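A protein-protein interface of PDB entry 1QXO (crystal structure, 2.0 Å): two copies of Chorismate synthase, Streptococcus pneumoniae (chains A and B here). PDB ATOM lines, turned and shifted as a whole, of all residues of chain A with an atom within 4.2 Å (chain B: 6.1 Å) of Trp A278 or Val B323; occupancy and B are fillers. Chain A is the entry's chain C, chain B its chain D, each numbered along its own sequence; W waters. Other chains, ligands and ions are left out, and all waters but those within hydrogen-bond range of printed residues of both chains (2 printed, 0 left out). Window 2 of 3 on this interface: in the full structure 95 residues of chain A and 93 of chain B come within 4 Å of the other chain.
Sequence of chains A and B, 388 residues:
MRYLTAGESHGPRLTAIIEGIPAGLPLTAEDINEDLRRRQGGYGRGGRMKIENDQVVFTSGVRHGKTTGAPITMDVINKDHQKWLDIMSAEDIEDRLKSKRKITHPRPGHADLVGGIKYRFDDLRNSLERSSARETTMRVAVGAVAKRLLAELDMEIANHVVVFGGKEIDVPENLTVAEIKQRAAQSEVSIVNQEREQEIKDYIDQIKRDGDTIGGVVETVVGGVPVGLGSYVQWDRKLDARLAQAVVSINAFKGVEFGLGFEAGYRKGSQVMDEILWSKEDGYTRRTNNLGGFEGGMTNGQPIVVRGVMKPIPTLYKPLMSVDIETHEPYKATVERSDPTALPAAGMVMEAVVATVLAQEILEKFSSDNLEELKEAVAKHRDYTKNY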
ATOM      1  N   ILE A 276     -27.837 -24.371  23.851  1.00  0.00           N
ATOM      2  CA  ILE A 276     -27.866 -23.456  22.718  1.00  0.00           C
ATOM      3  C   ILE A 276     -26.702 -22.457  22.793  1.00  0.00           C
ATOM      4  O   ILE A 276     -26.643 -21.774  23.811  1.00  0.00           O
ATOM      5  CB  ILE A 276     -29.222 -22.738  22.656  1.00  0.00           C
ATOM      6  CG1 ILE A 276     -30.358 -23.786  22.456  1.00  0.00           C
ATOM      7  CG2 ILE A 276     -29.313 -21.680  21.572  1.00  0.00           C
ATOM      8  CD1 ILE A 276     -31.727 -23.128  22.651  1.00  0.00           C
ATOM      9  N   LEU A 277     -25.912 -22.399  21.750  1.00  0.00           N
ATOM     10  CA  LEU A 277     -24.769 -21.475  21.658  1.00  0.00           C
ATOM     11  C   LEU A 277     -24.960 -20.523  20.468  1.00  0.00           C
ATOM     12  O   LEU A 277     -25.632 -20.846  19.472  1.00  0.00           O
ATOM     13  CB  LEU A 277     -23.497 -22.270  21.358  1.00  0.00           C
ATOM     14  CG  LEU A 277     -23.066 -23.300  22.414  1.00  0.00           C
ATOM     15  CD1 LEU A 277     -21.981 -24.239  21.874  1.00  0.00           C
ATOM     16  CD2 LEU A 277     -22.656 -22.570  23.684  1.00  0.00           C
ATOM     17  N   TRP A 278     -24.209 -19.434  20.438  1.00  0.00           N
ATOM     18  CA  TRP A 278     -24.329 -18.427  19.390  1.00  0.00           C
ATOM     19  C   TRP A 278     -22.965 -17.774  19.194  1.00  0.00           C
ATOM     20  O   TRP A 278     -22.271 -17.557  20.193  1.00  0.00           O
ATOM     21  CB  TRP A 278     -25.367 -17.337  19.760  1.00  0.00           C
ATOM     22  CG  TRP A 278     -25.516 -16.303  18.679  1.00  0.00           C
ATOM     23  CD1 TRP A 278     -26.391 -16.323  17.625  1.00  0.00           C
ATOM     24  CD2 TRP A 278     -24.761 -15.097  18.511  1.00  0.00           C
ATOM     25  NE1 TRP A 278     -26.216 -15.238  16.813  1.00  0.00           N
ATOM     26  CE2 TRP A 278     -25.237 -14.450  17.359  1.00  0.00           C
ATOM     27  CE3 TRP A 278     -23.711 -14.508  19.226  1.00  0.00           C
ATOM     28  CZ2 TRP A 278     -24.678 -13.261  16.862  1.00  0.00           C
ATOM     29  CZ3 TRP A 278     -23.160 -13.331  18.749  1.00  0.00           C
ATOM     30  CH2 TRP A 278     -23.674 -12.704  17.602  1.00  0.00           C
ATOM     31  N   SER A 279     -22.612 -17.409  17.990  1.00  0.00           N
ATOM     32  CA  SER A 279     -21.338 -16.765  17.708  1.00  0.00           C
ATOM     33  C   SER A 279     -21.618 -15.848  16.516  1.00  0.00           C
ATOM     34  O   SER A 279     -22.474 -16.203  15.707  1.00  0.00           O
ATOM     35  CB  SER A 279     -20.236 -17.753  17.325  1.00  0.00           C
ATOM     36  OG  SER A 279     -20.351 -18.167  15.977  1.00  0.00           O
ATOM     37  N   LYS A 280     -20.893 -14.759  16.402  1.00  0.00           N
ATOM     38  CA  LYS A 280     -21.120 -13.824  15.305  1.00  0.00           C
ATOM     39  C   LYS A 280     -20.764 -14.505  13.991  1.00  0.00           C
ATOM     40  O   LYS A 280     -21.353 -14.263  12.937  1.00  0.00           O
ATOM     41  CB  LYS A 280     -20.286 -12.544  15.491  1.00  0.00           C
ATOM     42  CG  LYS A 280     -18.819 -12.809  15.803  1.00  0.00           C
ATOM     43  CD  LYS A 280     -17.888 -11.706  15.316  1.00  0.00           C
ATOM     44  CE  LYS A 280     -16.467 -11.905  15.839  1.00  0.00           C
ATOM     45  NZ  LYS A 280     -15.543 -10.839  15.342  1.00  0.00           N
ATOM     46  N   GLY A 283     -23.699 -17.812  13.875  1.00  0.00           N
ATOM     47  CA  GLY A 283     -25.134 -17.798  14.272  1.00  0.00           C
ATOM     48  C   GLY A 283     -25.327 -18.874  15.353  1.00  0.00           C
ATOM     49  O   GLY A 283     -24.379 -19.138  16.143  1.00  0.00           O
ATOM     50  N   TYR A 284     -26.542 -19.374  15.455  1.00  0.00           N
ATOM     51  CA  TYR A 284     -26.905 -20.350  16.455  1.00  0.00           C
ATOM     52  C   TYR A 284     -26.420 -21.751  16.126  1.00  0.00           C
ATOM     53  O   TYR A 284     -26.376 -22.158  14.970  1.00  0.00           O
ATOM     54  CB  TYR A 284     -28.408 -20.455  16.735  1.00  0.00           C
ATOM     55  CG  TYR A 284     -28.969 -19.221  17.403  1.00  0.00           C
ATOM     56  CD1 TYR A 284     -29.447 -18.156  16.628  1.00  0.00           C
ATOM     57  CD2 TYR A 284     -28.975 -19.096  18.780  1.00  0.00           C
ATOM     58  CE1 TYR A 284     -29.919 -17.025  17.258  1.00  0.00           C
ATOM     59  CE2 TYR A 284     -29.433 -17.954  19.406  1.00  0.00           C
ATOM     60  CZ  TYR A 284     -29.941 -16.931  18.632  1.00  0.00           C
ATOM     61  OH  TYR A 284     -30.454 -15.814  19.249  1.00  0.00           O
ATOM     62  N   THR B 104     -37.882 -14.479  25.352  1.00  0.00           N
ATOM     63  CA  THR B 104     -36.701 -14.255  24.517  1.00  0.00           C
ATOM     64  C   THR B 104     -35.579 -15.224  24.873  1.00  0.00           C
ATOM     65  O   THR B 104     -34.479 -15.097  24.327  1.00  0.00           O
ATOM     66  CB  THR B 104     -36.137 -12.824  24.741  1.00  0.00           C
ATOM     67  OG1 THR B 104     -36.029 -12.643  26.168  1.00  0.00           O
ATOM     68  CG2 THR B 104     -37.065 -11.769  24.167  1.00  0.00           C
ATOM     69  N   HIS B 105     -35.802 -16.171  25.779  1.00  0.00           N
ATOM     70  CA  HIS B 105     -34.725 -17.087  26.214  1.00  0.00           C
ATOM     71  C   HIS B 105     -35.204 -18.497  25.882  1.00  0.00           C
ATOM     72  O   HIS B 105     -35.968 -19.095  26.642  1.00  0.00           O
ATOM     73  CB  HIS B 105     -34.444 -16.978  27.724  1.00  0.00           C
ATOM     74  CG  HIS B 105     -34.047 -15.587  28.104  1.00  0.00           C
ATOM     75  ND1 HIS B 105     -34.672 -14.835  29.063  1.00  0.00           N
ATOM     76  CD2 HIS B 105     -33.078 -14.789  27.584  1.00  0.00           C
ATOM     77  CE1 HIS B 105     -34.109 -13.634  29.135  1.00  0.00           C
ATOM     78  NE2 HIS B 105     -33.133 -13.579  28.248  1.00  0.00           N
ATOM     79  N   PRO B 106     -34.792 -19.008  24.710  1.00  0.00           N
ATOM     80  CA  PRO B 106     -35.243 -20.303  24.264  1.00  0.00           C
ATOM     81  C   PRO B 106     -34.817 -21.449  25.141  1.00  0.00           C
ATOM     82  O   PRO B 106     -33.684 -21.512  25.615  1.00  0.00           O
ATOM     83  CB  PRO B 106     -34.711 -20.386  22.835  1.00  0.00           C
ATOM     84  CG  PRO B 106     -33.482 -19.506  22.887  1.00  0.00           C
ATOM     85  CD  PRO B 106     -33.912 -18.343  23.753  1.00  0.00           C
ATOM     86  N   MET B 321     -27.652 -23.825  29.623  1.00  0.00           N
ATOM     87  CA  MET B 321     -27.288 -22.586  28.923  1.00  0.00           C
ATOM     88  C   MET B 321     -28.067 -22.391  27.623  1.00  0.00           C
ATOM     89  O   MET B 321     -28.287 -23.298  26.838  1.00  0.00           O
ATOM     90  CB  MET B 321     -25.805 -22.541  28.580  1.00  0.00           C
ATOM     91  CG  MET B 321     -24.887 -22.661  29.799  1.00  0.00           C
ATOM     92  SD  MET B 321     -25.293 -20.928  30.732  1.00  0.00           S
ATOM     93  CE  MET B 321     -25.397 -19.501  29.368  1.00  0.00           C
ATOM     94  N   SER B 322     -28.411 -21.149  27.371  1.00  0.00           N
ATOM     95  CA  SER B 322     -29.079 -20.731  26.146  1.00  0.00           C
ATOM     96  C   SER B 322     -28.565 -19.364  25.711  1.00  0.00           C
ATOM     97  O   SER B 322     -27.490 -18.931  26.166  1.00  0.00           O
ATOM     98  CB  SER B 322     -30.582 -20.653  26.389  1.00  0.00           C
ATOM     99  OG  SER B 322     -31.278 -20.552  25.158  1.00  0.00           O
ATOM    100  N   VAL B 323     -29.321 -18.723  24.832  1.00  0.00           N
ATOM    101  CA  VAL B 323     -28.984 -17.392  24.355  1.00  0.00           C
ATOM    102  C   VAL B 323     -30.238 -16.525  24.309  1.00  0.00           C
ATOM    103  O   VAL B 323     -31.314 -17.021  23.959  1.00  0.00           O
ATOM    104  CB  VAL B 323     -28.354 -17.476  22.952  1.00  0.00           C
ATOM    105  CG1 VAL B 323     -28.021 -16.106  22.373  1.00  0.00           C
ATOM    106  CG2 VAL B 323     -27.168 -18.393  22.986  1.00  0.00           C
ATOM    107  N   ASP B 324     -30.115 -15.262  24.682  1.00  0.00           N
ATOM    108  CA  ASP B 324     -31.123 -14.241  24.678  1.00  0.00           C
ATOM    109  C   ASP B 324     -31.231 -13.763  23.206  1.00  0.00           C
ATOM    110  O   ASP B 324     -30.243 -13.217  22.683  1.00  0.00           O
ATOM    111  CB  ASP B 324     -30.732 -13.076  25.581  1.00  0.00           C
ATOM    112  CG  ASP B 324     -31.695 -11.930  25.707  1.00  0.00           C
ATOM    113  OD1 ASP B 324     -31.919 -11.512  26.870  1.00  0.00           O
ATOM    114  OD2 ASP B 324     -32.224 -11.404  24.711  1.00  0.00           O
ATOM    115  N   ILE B 325     -32.428 -13.998  22.658  1.00  0.00           N
ATOM    116  CA  ILE B 325     -32.603 -13.741  21.238  1.00  0.00           C
ATOM    117  C   ILE B 325     -32.516 -12.267  20.896  1.00  0.00           C
ATOM    118  O   ILE B 325     -32.192 -11.995  19.733  1.00  0.00           O
ATOM    119  CB  ILE B 325     -33.863 -14.417  20.670  1.00  0.00           C
ATOM    120  CG1 ILE B 325     -35.162 -13.793  21.216  1.00  0.00           C
ATOM    121  CG2 ILE B 325     -33.830 -15.896  21.010  1.00  0.00           C
ATOM    122  CD1 ILE B 325     -36.415 -14.264  20.489  1.00  0.00           C
ATOM    123  N   THR B 327     -30.418 -10.029  22.609  1.00  0.00           N
ATOM    124  CA  THR B 327     -29.064  -9.468  22.762  1.00  0.00           C
ATOM    125  C   THR B 327     -27.988 -10.366  22.174  1.00  0.00           C
ATOM    126  O   THR B 327     -26.861  -9.911  22.004  1.00  0.00           O
ATOM    127  CB  THR B 327     -28.715  -9.299  24.254  1.00  0.00           C
ATOM    128  OG1 THR B 327     -28.792 -10.621  24.799  1.00  0.00           O
ATOM    129  CG2 THR B 327     -29.651  -8.355  24.981  1.00  0.00           C
ATOM    130  N   HIS B 328     -28.305 -11.644  21.948  1.00  0.00           N
ATOM    131  CA  HIS B 328     -27.318 -12.619  21.538  1.00  0.00           C
ATOM    132  C   HIS B 328     -26.333 -12.965  22.656  1.00  0.00           C
ATOM    133  O   HIS B 328     -25.304 -13.610  22.402  1.00  0.00           O
ATOM    134  CB  HIS B 328     -26.549 -12.191  20.295  1.00  0.00           C
ATOM    135  CG  HIS B 328     -27.393 -12.346  19.064  1.00  0.00           C
ATOM    136  ND1 HIS B 328     -27.364 -11.448  18.037  1.00  0.00           N
ATOM    137  CD2 HIS B 328     -28.288 -13.308  18.733  1.00  0.00           C
ATOM    138  CE1 HIS B 328     -28.202 -11.855  17.088  1.00  0.00           C
ATOM    139  NE2 HIS B 328     -28.782 -12.976  17.503  1.00  0.00           N
ATOM    140  N   GLU B 329     -26.657 -12.634  23.892  1.00  0.00           N
ATOM    141  CA  GLU B 329     -25.760 -12.973  25.010  1.00  0.00           C
ATOM    142  C   GLU B 329     -26.227 -14.280  25.631  1.00  0.00           C
ATOM    143  O   GLU B 329     -27.440 -14.543  25.641  1.00  0.00           O
ATOM    144  CB  GLU B 329     -25.795 -11.847  26.030  1.00  0.00           C
ATOM    145  CG  GLU B 329     -25.139 -10.552  25.590  1.00  0.00           C
ATOM    146  CD  GLU B 329     -23.633 -10.691  25.530  1.00  0.00           C
ATOM    147  OE1 GLU B 329     -23.072 -11.100  26.573  1.00  0.00           O
ATOM    148  OE2 GLU B 329     -23.053 -10.433  24.456  1.00  0.00           O
ATOM    149  N   PRO B 330     -25.302 -15.111  26.100  1.00  0.00           N
ATOM    150  CA  PRO B 330     -25.671 -16.358  26.751  1.00  0.00           C
ATOM    151  C   PRO B 330     -26.421 -16.033  28.035  1.00  0.00           C
ATOM    152  O   PRO B 330     -26.255 -14.952  28.607  1.00  0.00           O
ATOM    153  CB  PRO B 330     -24.373 -17.092  26.997  1.00  0.00           C
ATOM    154  CG  PRO B 330     -23.290 -16.119  26.768  1.00  0.00           C
ATOM    155  CD  PRO B 330     -23.860 -14.857  26.180  1.00  0.00           C
ATOM    156  N   TYR B 331     -27.233 -16.969  28.469  1.00  0.00           N
ATOM    157  CA  TYR B 331     -28.067 -16.837  29.646  1.00  0.00           C
ATOM    158  C   TYR B 331     -28.657 -18.213  29.954  1.00  0.00           C
ATOM    159  O   TYR B 331     -28.583 -19.134  29.129  1.00  0.00           O
ATOM    160  CB  TYR B 331     -29.229 -15.957  29.205  1.00  0.00           C
ATOM    161  CG  TYR B 331     -29.824 -14.889  30.062  1.00  0.00           C
ATOM    162  CD1 TYR B 331     -29.396 -13.566  29.957  1.00  0.00           C
ATOM    163  CD2 TYR B 331     -30.833 -15.163  30.979  1.00  0.00           C
ATOM    164  CE1 TYR B 331     -29.936 -12.562  30.739  1.00  0.00           C
ATOM    165  CE2 TYR B 331     -31.386 -14.171  31.767  1.00  0.00           C
ATOM    166  CZ  TYR B 331     -30.931 -12.871  31.643  1.00  0.00           C
ATOM    167  OH  TYR B 331     -31.482 -11.875  32.432  1.00  0.00           O
ATOM    168  N   LYS B 332     -29.267 -18.335  31.118  1.00  0.00           N
ATOM    169  CA  LYS B 332     -29.909 -19.620  31.452  1.00  0.00           C
ATOM    170  C   LYS B 332     -31.219 -19.649  30.663  1.00  0.00           C
ATOM    171  O   LYS B 332     -31.721 -18.602  30.208  1.00  0.00           O
ATOM    172  CB  LYS B 332     -30.019 -19.724  32.967  1.00  0.00           C
ATOM    173  CG  LYS B 332     -28.614 -19.984  33.523  1.00  0.00           C
ATOM    174  CD  LYS B 332     -28.505 -19.989  35.032  1.00  0.00           C
ATOM    175  CE  LYS B 332     -27.374 -20.868  35.545  1.00  0.00           C
ATOM    176  NZ  LYS B 332     -26.223 -20.938  34.618  1.00  0.00           N
HETATM  177  O   HOH W   1     -25.076 -20.093  25.284  1.00  0.00           O
HETATM  178  O   HOH W   2     -31.553 -13.804  17.902  1.00  0.00           O
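NE1 of Trp A278 lies close to NE2 of His B328 (3.5 Å). O of Met B321 is in hydrogen-bond range of N of Ile A276.
The backbone carbonyl oxygen (O) of Thr B104 sits at hydrogen-bond distance from the backbone NH (N) of Ile B325 (2.9 Å). O of Pro B106 is in hydrogen-bond range of OG of Ser B322. N of Ser B322 is in hydrogen-bond range of O of Tyr B331 (2.7 Å).
O of Pro B106 touches CD1 of Ile A276 (3.9 Å). Ile A276 touches Ser B322 (O to CA, 3.5 Å). Ile A276 touches Val B323. Leu A277 touches Val B323. Trp A278 touches Val B323 (CB to CG2, 3.8 Å). Tyr A284 touches Val B323. Ile B325 touches Tyr A284 (CA to OH, 3.6 Å). His B328 touches Tyr A284.
Of the printed residues of chain A, Val B323 touches Ile A276 (3.5 Å), Leu A277 (3.97 Å), Trp A278 (3.8 Å) and Tyr A284 (3.7 Å). Printed residues of chain A within 4 Å of Ile B325: Tyr A284 (3.6 Å). Of the printed residues of chain B, Ile A276 touches Pro B106 (3.9 Å), Met B321 (3.2 Å), Ser B322 (3.5 Å) and Val B323 (3.5 Å). Of the printed residues of chain A, Ser B322 touches Ile A276. Printed residues of chain B within 4 Å of Leu A277: Val B323 (3.97 Å). Of the printed residues of chain B, Tyr A284 touches Val B323, Ile B325 and His B328. Thr B327 touches none of the printed residues of chain A. The nearest residue of chain B that does not touch Trp A278 is Glu B329 (5.8 Å). The nearest printed residue of chain A that does not touch Val B323 is Ser A279 (6.8 Å).
Among the printed residues, 10 pairs touch across the chains. Among the printed residues, no Asp or Glu carboxylate lies within 4 Å of a Lys or Arg side-chain nitrogen of the other chain.
No position is printed for both chains. Of the 10 pairs that touch across the chains among the printed residues, none has its exchanged pair printed and touching as well.
Water W2 lies within hydrogen-bond range of O of Ile B325 (2.7 Å), OH of Tyr A284 (2.7 Å) and NE2 of His B328 (2.9 Å). Water W1 lies within hydrogen-bond range of the backbone carbonyl oxygen of Ile A276 (2.7 Å) and the backbone carbonyl oxygen of Ser B322 (2.8 Å).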
